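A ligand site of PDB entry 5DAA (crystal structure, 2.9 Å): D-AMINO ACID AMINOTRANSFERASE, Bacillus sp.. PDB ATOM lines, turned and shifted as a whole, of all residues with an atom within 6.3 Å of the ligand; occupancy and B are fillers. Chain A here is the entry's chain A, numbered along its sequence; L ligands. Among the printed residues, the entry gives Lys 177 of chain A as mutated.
N of Ile 204 sits at hydrogen-bond distance from O3 of the ligand, at 2.7 Å.
N1 of the ligand is in hydrogen-bond range of N of Ser 181, 3.4 Å away.
The guanidinium group (NH2) of Arg 50 is in salt-bridge range of an oxygen (O3) of the ligand, 2.9 Å away.
The side-chain hydroxyl of Thr 205 is in hydrogen-bond range of an oxygen (O5) of the ligand.
O4 of the ligand is in hydrogen-bond range of OG1 of Thr 241, 2.7 Å away.
The backbone NH (N) of Thr 205 sits at hydrogen-bond distance from an oxygen (O5) of the ligand, at 3.1 Å.
The backbone NH (N) of Thr 241 is in hydrogen-bond range of an oxygen (O4) of the ligand, at 3.0 Å.
NZ of Lys 145 is bonded to C5 of the ligand.
ND1 of His 47 sits at hydrogen-bond distance from OE1 of Glu 32 (2.9 Å).
The guanidinium group (NH1) of Arg 50 sits at hydrogen-bond distance from the backbone carbonyl oxygen (O) of Lys 202, 3.0 Å away.
The guanidinium group (NH2) of Arg 50 lies within salt-bridge range of the side-chain carboxylate (OE1) of Glu 32 (2.9 Å).
The backbone NH (N) of Tyr 31 lies within hydrogen-bond range of the backbone carbonyl oxygen (O) of Lys 145, at 3.1 Å.
The backbone NH (N) of Leu 201 lies close to the backbone carbonyl oxygen (O) of Cys 142, 3.4 Å away.
O of Ser 240 lies close to OG1 of Thr 205 (3.3 Å).
N of Thr 241 lies within hydrogen-bond range of OG1 of Thr 205 (3.2 Å).
O of Asn 182 is in hydrogen-bond range of N of Thr 239 (2.9 Å).
Merely in contact with the ligand: His 47 (3.9 Å), Ser 180 (3.9 Å), Asn 182 (3.9 Å), Leu 201 (3.5 Å), Gly 203 (3.3 Å) and Ser 240 (3.4 Å).
The nearest printed residue that does not touch the ligand is Tyr 31 (4.03 Å).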
ATOM      1  N   TYR A  31       5.558 -27.326   2.451  1.00  0.00           N
ATOM      2  CA  TYR A  31       5.466 -27.854   3.822  1.00  0.00           C
ATOM      3  C   TYR A  31       5.369 -26.773   4.905  1.00  0.00           C
ATOM      4  O   TYR A  31       5.318 -25.571   4.620  1.00  0.00           O
ATOM      5  CB  TYR A  31       6.652 -28.779   4.115  1.00  0.00           C
ATOM      6  CG  TYR A  31       7.952 -28.053   4.336  1.00  0.00           C
ATOM      7  CD1 TYR A  31       8.732 -27.657   3.258  1.00  0.00           C
ATOM      8  CD2 TYR A  31       8.401 -27.749   5.625  1.00  0.00           C
ATOM      9  CE1 TYR A  31       9.916 -26.961   3.448  1.00  0.00           C
ATOM     10  CE2 TYR A  31       9.585 -27.051   5.829  1.00  0.00           C
ATOM     11  CZ  TYR A  31      10.344 -26.656   4.730  1.00  0.00           C
ATOM     12  OH  TYR A  31      11.515 -25.965   4.900  1.00  0.00           O
ATOM     13  N   GLU A  32       5.312 -27.234   6.156  1.00  0.00           N
ATOM     14  CA  GLU A  32       5.245 -26.380   7.348  1.00  0.00           C
ATOM     15  C   GLU A  32       5.755 -27.195   8.528  1.00  0.00           C
ATOM     16  O   GLU A  32       5.895 -28.422   8.422  1.00  0.00           O
ATOM     17  CB  GLU A  32       3.814 -25.942   7.674  1.00  0.00           C
ATOM     18  CG  GLU A  32       3.194 -24.884   6.762  1.00  0.00           C
ATOM     19  CD  GLU A  32       3.924 -23.550   6.798  1.00  0.00           C
ATOM     20  OE1 GLU A  32       4.347 -23.095   7.883  1.00  0.00           O
ATOM     21  OE2 GLU A  32       4.051 -22.954   5.710  1.00  0.00           O
ATOM     22  N   VAL A  33       6.038 -26.508   9.625  1.00  0.00           N
ATOM     23  CA  VAL A  33       6.500 -27.153  10.841  1.00  0.00           C
ATOM     24  C   VAL A  33       5.975 -26.329  12.011  1.00  0.00           C
ATOM     25  O   VAL A  33       6.351 -25.171  12.177  1.00  0.00           O
ATOM     26  CB  VAL A  33       8.047 -27.245  10.917  1.00  0.00           C
ATOM     27  CG1 VAL A  33       8.473 -27.806  12.270  1.00  0.00           C
ATOM     28  CG2 VAL A  33       8.570 -28.144   9.825  1.00  0.00           C
ATOM     29  N   HIS A  47       0.209 -20.846  10.345  1.00  0.00           N
ATOM     30  CA  HIS A  47       0.954 -21.852   9.592  1.00  0.00           C
ATOM     31  C   HIS A  47       0.116 -22.513   8.492  1.00  0.00           C
ATOM     32  O   HIS A  47       0.623 -22.761   7.400  1.00  0.00           O
ATOM     33  CB  HIS A  47       1.546 -22.913  10.540  1.00  0.00           C
ATOM     34  CG  HIS A  47       2.823 -22.499  11.207  1.00  0.00           C
ATOM     35  ND1 HIS A  47       4.067 -22.844  10.723  1.00  0.00           N
ATOM     36  CD2 HIS A  47       3.050 -21.747  12.308  1.00  0.00           C
ATOM     37  CE1 HIS A  47       4.993 -22.326  11.496  1.00  0.00           C
ATOM     38  NE2 HIS A  47       4.412 -21.659  12.469  1.00  0.00           N
ATOM     39  N   ARG A  50      -0.251 -20.228   5.500  1.00  0.00           N
ATOM     40  CA  ARG A  50       0.963 -20.147   4.695  1.00  0.00           C
ATOM     41  C   ARG A  50       1.159 -21.422   3.895  1.00  0.00           C
ATOM     42  O   ARG A  50       1.857 -21.426   2.883  1.00  0.00           O
ATOM     43  CB  ARG A  50       2.187 -19.905   5.570  1.00  0.00           C
ATOM     44  CG  ARG A  50       3.452 -19.621   4.774  1.00  0.00           C
ATOM     45  CD  ARG A  50       4.579 -19.151   5.676  1.00  0.00           C
ATOM     46  NE  ARG A  50       5.037 -20.194   6.592  1.00  0.00           N
ATOM     47  CZ  ARG A  50       6.027 -20.029   7.459  1.00  0.00           C
ATOM     48  NH1 ARG A  50       6.669 -18.877   7.532  1.00  0.00           N
ATOM     49  NH2 ARG A  50       6.391 -21.036   8.233  1.00  0.00           N
ATOM     50  N   ARG A 138      20.786 -20.363  -3.502  1.00  0.00           N
ATOM     51  CA  ARG A 138      19.458 -20.972  -3.599  1.00  0.00           C
ATOM     52  C   ARG A 138      18.634 -20.379  -4.748  1.00  0.00           C
ATOM     53  O   ARG A 138      18.972 -19.315  -5.269  1.00  0.00           O
ATOM     54  CB  ARG A 138      18.685 -20.805  -2.292  1.00  0.00           C
ATOM     55  CG  ARG A 138      19.417 -21.260  -1.057  1.00  0.00           C
ATOM     56  CD  ARG A 138      18.462 -21.415   0.110  1.00  0.00           C
ATOM     57  NE  ARG A 138      17.614 -22.604  -0.035  1.00  0.00           N
ATOM     58  CZ  ARG A 138      16.293 -22.611   0.084  1.00  0.00           C
ATOM     59  NH1 ARG A 138      15.630 -21.486   0.358  1.00  0.00           N
ATOM     60  NH2 ARG A 138      15.620 -23.744  -0.028  1.00  0.00           N
ATOM     61  N   CYS A 142      12.279 -18.192  -2.650  1.00  0.00           N
ATOM     62  CA  CYS A 142      12.263 -18.551  -1.243  1.00  0.00           C
ATOM     63  C   CYS A 142      11.069 -17.987  -0.502  1.00  0.00           C
ATOM     64  O   CYS A 142      10.890 -18.236   0.693  1.00  0.00           O
ATOM     65  CB  CYS A 142      13.553 -18.110  -0.567  1.00  0.00           C
ATOM     66  SG  CYS A 142      14.943 -19.070  -1.135  1.00  0.00           S
ATOM     67  N   LYS A 145       7.707 -21.826   0.814  1.00  0.00           N
ATOM     68  CA  LYS A 145       8.332 -22.845   1.640  1.00  0.00           C
ATOM     69  C   LYS A 145       8.128 -24.194   0.939  1.00  0.00           C
ATOM     70  O   LYS A 145       7.252 -24.988   1.316  1.00  0.00           O
ATOM     71  CB  LYS A 145       7.706 -22.855   3.048  1.00  0.00           C
ATOM     72  CG  LYS A 145       8.542 -23.525   4.117  1.00  0.00           C
ATOM     73  CD  LYS A 145       7.890 -23.357   5.474  1.00  0.00           C
ATOM     74  CE  LYS A 145       8.917 -23.442   6.625  1.00  0.00           C
ATOM     75  NZ  LYS A 145       9.937 -22.398   6.514  1.00  0.00           N
ATOM     76  N   LEU A 149      15.076 -27.924  -1.236  1.00  0.00           N
ATOM     77  CA  LEU A 149      15.958 -27.501  -0.154  1.00  0.00           C
ATOM     78  C   LEU A 149      17.420 -27.902  -0.206  1.00  0.00           C
ATOM     79  O   LEU A 149      18.109 -27.769   0.802  1.00  0.00           O
ATOM     80  CB  LEU A 149      15.394 -28.007   1.171  1.00  0.00           C
ATOM     81  CG  LEU A 149      13.976 -27.603   1.531  1.00  0.00           C
ATOM     82  CD1 LEU A 149      13.312 -28.678   2.333  1.00  0.00           C
ATOM     83  CD2 LEU A 149      14.030 -26.294   2.282  1.00  0.00           C
ATOM     84  N   LYS A 177      19.163 -14.349   4.833  1.00  0.00           N
ATOM     85  CA  LYS A 177      18.494 -15.215   5.802  1.00  0.00           C
ATOM     86  C   LYS A 177      19.453 -16.366   6.147  1.00  0.00           C
ATOM     87  O   LYS A 177      20.483 -16.541   5.493  1.00  0.00           O
ATOM     88  CB  LYS A 177      17.278 -15.836   5.119  1.00  0.00           C
ATOM     89  CG  LYS A 177      17.741 -16.727   3.982  1.00  0.00           C
ATOM     90  CD  LYS A 177      16.766 -16.925   2.863  1.00  0.00           C
ATOM     91  CE  LYS A 177      17.599 -17.245   1.624  1.00  0.00           C
ATOM     92  NZ  LYS A 177      16.939 -18.018   0.542  1.00  0.00           N
ATOM     93  N   GLY A 178      19.079 -17.189   7.115  1.00  0.00           N
ATOM     94  CA  GLY A 178      19.897 -18.327   7.473  1.00  0.00           C
ATOM     95  C   GLY A 178      19.461 -19.516   6.624  1.00  0.00           C
ATOM     96  O   GLY A 178      18.485 -19.400   5.877  1.00  0.00           O
ATOM     97  N   SER A 179      20.166 -20.651   6.724  1.00  0.00           N
ATOM     98  CA  SER A 179      19.805 -21.837   5.946  1.00  0.00           C
ATOM     99  C   SER A 179      18.357 -22.229   6.222  1.00  0.00           C
ATOM    100  O   SER A 179      17.628 -22.594   5.303  1.00  0.00           O
ATOM    101  CB  SER A 179      20.724 -23.028   6.263  1.00  0.00           C
ATOM    102  OG  SER A 179      20.396 -23.637   7.496  1.00  0.00           O
ATOM    103  N   SER A 180      17.942 -22.103   7.478  1.00  0.00           N
ATOM    104  CA  SER A 180      16.573 -22.412   7.877  1.00  0.00           C
ATOM    105  C   SER A 180      16.038 -21.512   8.976  1.00  0.00           C
ATOM    106  O   SER A 180      15.405 -21.996   9.911  1.00  0.00           O
ATOM    107  CB  SER A 180      16.449 -23.878   8.298  1.00  0.00           C
ATOM    108  OG  SER A 180      17.358 -24.202   9.339  1.00  0.00           O
ATOM    109  N   SER A 181      16.261 -20.199   8.838  1.00  0.00           N
ATOM    110  CA  SER A 181      15.813 -19.198   9.813  1.00  0.00           C
ATOM    111  C   SER A 181      15.921 -17.759   9.267  1.00  0.00           C
ATOM    112  O   SER A 181      16.508 -17.533   8.203  1.00  0.00           O
ATOM    113  CB  SER A 181      16.698 -19.279  11.057  1.00  0.00           C
ATOM    114  OG  SER A 181      18.045 -19.021  10.717  1.00  0.00           O
ATOM    115  N   ASN A 182      15.355 -16.806  10.000  1.00  0.00           N
ATOM    116  CA  ASN A 182      15.421 -15.400   9.617  1.00  0.00           C
ATOM    117  C   ASN A 182      16.475 -14.729  10.499  1.00  0.00           C
ATOM    118  O   ASN A 182      16.635 -15.096  11.663  1.00  0.00           O
ATOM    119  CB  ASN A 182      14.072 -14.702   9.813  1.00  0.00           C
ATOM    120  CG  ASN A 182      13.065 -15.079   8.745  1.00  0.00           C
ATOM    121  OD1 ASN A 182      11.869 -15.209   9.027  1.00  0.00           O
ATOM    122  ND2 ASN A 182      13.531 -15.253   7.519  1.00  0.00           N
ATOM    123  N   ILE A 200      13.706 -13.946   0.730  1.00  0.00           N
ATOM    124  CA  ILE A 200      13.527 -14.584   2.033  1.00  0.00           C
ATOM    125  C   ILE A 200      12.126 -15.135   2.242  1.00  0.00           C
ATOM    126  O   ILE A 200      11.155 -14.663   1.643  1.00  0.00           O
ATOM    127  CB  ILE A 200      13.766 -13.605   3.218  1.00  0.00           C
ATOM    128  CG1 ILE A 200      12.683 -12.520   3.242  1.00  0.00           C
ATOM    129  CG2 ILE A 200      15.127 -12.966   3.109  1.00  0.00           C
ATOM    130  CD1 ILE A 200      12.642 -11.768   4.544  1.00  0.00           C
ATOM    131  N   LEU A 201      12.037 -16.119   3.129  1.00  0.00           N
ATOM    132  CA  LEU A 201      10.764 -16.722   3.497  1.00  0.00           C
ATOM    133  C   LEU A 201      10.222 -15.867   4.654  1.00  0.00           C
ATOM    134  O   LEU A 201      10.923 -15.590   5.631  1.00  0.00           O
ATOM    135  CB  LEU A 201      10.969 -18.187   3.932  1.00  0.00           C
ATOM    136  CG  LEU A 201       9.744 -19.082   4.175  1.00  0.00           C
ATOM    137  CD1 LEU A 201       9.393 -19.143   5.641  1.00  0.00           C
ATOM    138  CD2 LEU A 201       8.545 -18.630   3.344  1.00  0.00           C
ATOM    139  N   LYS A 202       9.002 -15.387   4.506  1.00  0.00           N
ATOM    140  CA  LYS A 202       8.376 -14.564   5.532  1.00  0.00           C
ATOM    141  C   LYS A 202       7.911 -15.490   6.661  1.00  0.00           C
ATOM    142  O   LYS A 202       6.768 -15.974   6.658  1.00  0.00           O
ATOM    143  CB  LYS A 202       7.204 -13.791   4.913  1.00  0.00           C
ATOM    144  CG  LYS A 202       6.678 -12.641   5.735  1.00  0.00           C
ATOM    145  CD  LYS A 202       5.721 -11.803   4.882  1.00  0.00           C
ATOM    146  CE  LYS A 202       5.051 -10.693   5.682  1.00  0.00           C
ATOM    147  NZ  LYS A 202       3.981 -11.212   6.588  1.00  0.00           N
ATOM    148  N   GLY A 203       8.818 -15.748   7.605  1.00  0.00           N
ATOM    149  CA  GLY A 203       8.540 -16.622   8.732  1.00  0.00           C
ATOM    150  C   GLY A 203       7.538 -16.102   9.737  1.00  0.00           C
ATOM    151  O   GLY A 203       7.402 -14.896   9.933  1.00  0.00           O
ATOM    152  N   ILE A 204       6.846 -17.040  10.389  1.00  0.00           N
ATOM    153  CA  ILE A 204       5.846 -16.707  11.404  1.00  0.00           C
ATOM    154  C   ILE A 204       6.536 -16.191  12.664  1.00  0.00           C
ATOM    155  O   ILE A 204       6.109 -15.195  13.232  1.00  0.00           O
ATOM    156  CB  ILE A 204       4.947 -17.933  11.752  1.00  0.00           C
ATOM    157  CG1 ILE A 204       4.252 -18.482  10.483  1.00  0.00           C
ATOM    158  CG2 ILE A 204       3.918 -17.562  12.804  1.00  0.00           C
ATOM    159  CD1 ILE A 204       3.376 -17.510   9.772  1.00  0.00           C
ATOM    160  N   THR A 205       7.620 -16.860  13.088  1.00  0.00           N
ATOM    161  CA  THR A 205       8.349 -16.410  14.273  1.00  0.00           C
ATOM    162  C   THR A 205       8.901 -15.014  13.998  1.00  0.00           C
ATOM    163  O   THR A 205       8.931 -14.172  14.898  1.00  0.00           O
ATOM    164  CB  THR A 205       9.506 -17.378  14.652  1.00  0.00           C
ATOM    165  OG1 THR A 205       8.981 -18.688  14.891  1.00  0.00           O
ATOM    166  CG2 THR A 205      10.224 -16.892  15.917  1.00  0.00           C
ATOM    167  N   ARG A 206       9.300 -14.762  12.758  1.00  0.00           N
ATOM    168  CA  ARG A 206       9.822 -13.456  12.391  1.00  0.00           C
ATOM    169  C   ARG A 206       8.798 -12.363  12.707  1.00  0.00           C
ATOM    170  O   ARG A 206       9.108 -11.358  13.350  1.00  0.00           O
ATOM    171  CB  ARG A 206      10.153 -13.439  10.889  1.00  0.00           C
ATOM    172  CG  ARG A 206      10.529 -12.073  10.348  1.00  0.00           C
ATOM    173  CD  ARG A 206      10.414 -12.045   8.817  1.00  0.00           C
ATOM    174  NE  ARG A 206      10.958 -10.817   8.247  1.00  0.00           N
ATOM    175  CZ  ARG A 206      10.225  -9.841   7.736  1.00  0.00           C
ATOM    176  NH1 ARG A 206       8.909  -9.949   7.707  1.00  0.00           N
ATOM    177  NH2 ARG A 206      10.818  -8.763   7.256  1.00  0.00           N
ATOM    178  N   THR A 239      15.726 -16.446  14.017  1.00  0.00           N
ATOM    179  CA  THR A 239      14.405 -16.919  14.421  1.00  0.00           C
ATOM    180  C   THR A 239      13.844 -18.031  13.531  1.00  0.00           C
ATOM    181  O   THR A 239      14.221 -18.171  12.364  1.00  0.00           O
ATOM    182  CB  THR A 239      13.387 -15.755  14.446  1.00  0.00           C
ATOM    183  OG1 THR A 239      13.168 -15.270  13.120  1.00  0.00           O
ATOM    184  CG2 THR A 239      13.892 -14.621  15.340  1.00  0.00           C
ATOM    185  N   SER A 240      12.961 -18.827  14.116  1.00  0.00           N
ATOM    186  CA  SER A 240      12.289 -19.940  13.442  1.00  0.00           C
ATOM    187  C   SER A 240      11.389 -20.615  14.458  1.00  0.00           C
ATOM    188  O   SER A 240      11.591 -20.466  15.673  1.00  0.00           O
ATOM    189  CB  SER A 240      13.294 -20.972  12.943  1.00  0.00           C
ATOM    190  OG  SER A 240      13.825 -21.675  14.040  1.00  0.00           O
ATOM    191  N   THR A 241      10.426 -21.391  13.972  1.00  0.00           N
ATOM    192  CA  THR A 241       9.513 -22.088  14.857  1.00  0.00           C
ATOM    193  C   THR A 241      10.222 -22.935  15.912  1.00  0.00           C
ATOM    194  O   THR A 241       9.832 -22.902  17.083  1.00  0.00           O
ATOM    195  CB  THR A 241       8.492 -22.921  14.036  1.00  0.00           C
ATOM    196  OG1 THR A 241       7.727 -22.036  13.218  1.00  0.00           O
ATOM    197  CG2 THR A 241       7.537 -23.673  14.944  1.00  0.00           C
ATOM    198  N   THR A 242      11.300 -23.636  15.538  1.00  0.00           N
ATOM    199  CA  THR A 242      12.045 -24.498  16.474  1.00  0.00           C
ATOM    200  C   THR A 242      13.227 -23.885  17.237  1.00  0.00           C
ATOM    201  O   THR A 242      13.615 -24.394  18.295  1.00  0.00           O
ATOM    202  CB  THR A 242      12.508 -25.786  15.790  1.00  0.00           C
ATOM    203  OG1 THR A 242      13.071 -25.468  14.511  1.00  0.00           O
ATOM    204  CG2 THR A 242      11.347 -26.736  15.613  1.00  0.00           C
HETATM  205  N1  LIG L   1      13.677 -19.175   6.897  1.00  0.00           N
HETATM  206  C1  LIG L   1      13.587 -20.114   5.949  1.00  0.00           C
HETATM  207  C2  LIG L   1      14.531 -20.006   4.761  1.00  0.00           C
HETATM  208  C3  LIG L   1      12.598 -21.130   6.141  1.00  0.00           C
HETATM  209  O1  LIG L   1      12.542 -22.078   5.151  1.00  0.00           O
HETATM  210  C4  LIG L   1      11.775 -21.151   7.271  1.00  0.00           C
HETATM  211  C5  LIG L   1      10.772 -22.193   7.453  1.00  0.00           C
HETATM  212  C6  LIG L   1      11.987 -20.070   8.196  1.00  0.00           C
HETATM  213  C7  LIG L   1      12.918 -19.121   8.001  1.00  0.00           C
HETATM  214  C8  LIG L   1      11.199 -19.910   9.505  1.00  0.00           C
HETATM  215  O2  LIG L   1       9.836 -19.606   9.400  1.00  0.00           O
HETATM  216  P1  LIG L   1       9.060 -19.848  10.725  1.00  0.00           P
HETATM  217  O3  LIG L   1       7.622 -19.675  10.421  1.00  0.00           O
HETATM  218  O4  LIG L   1       9.322 -21.303  11.216  1.00  0.00           O
HETATM  219  O5  LIG L   1       9.577 -18.869  11.702  1.00  0.00           O
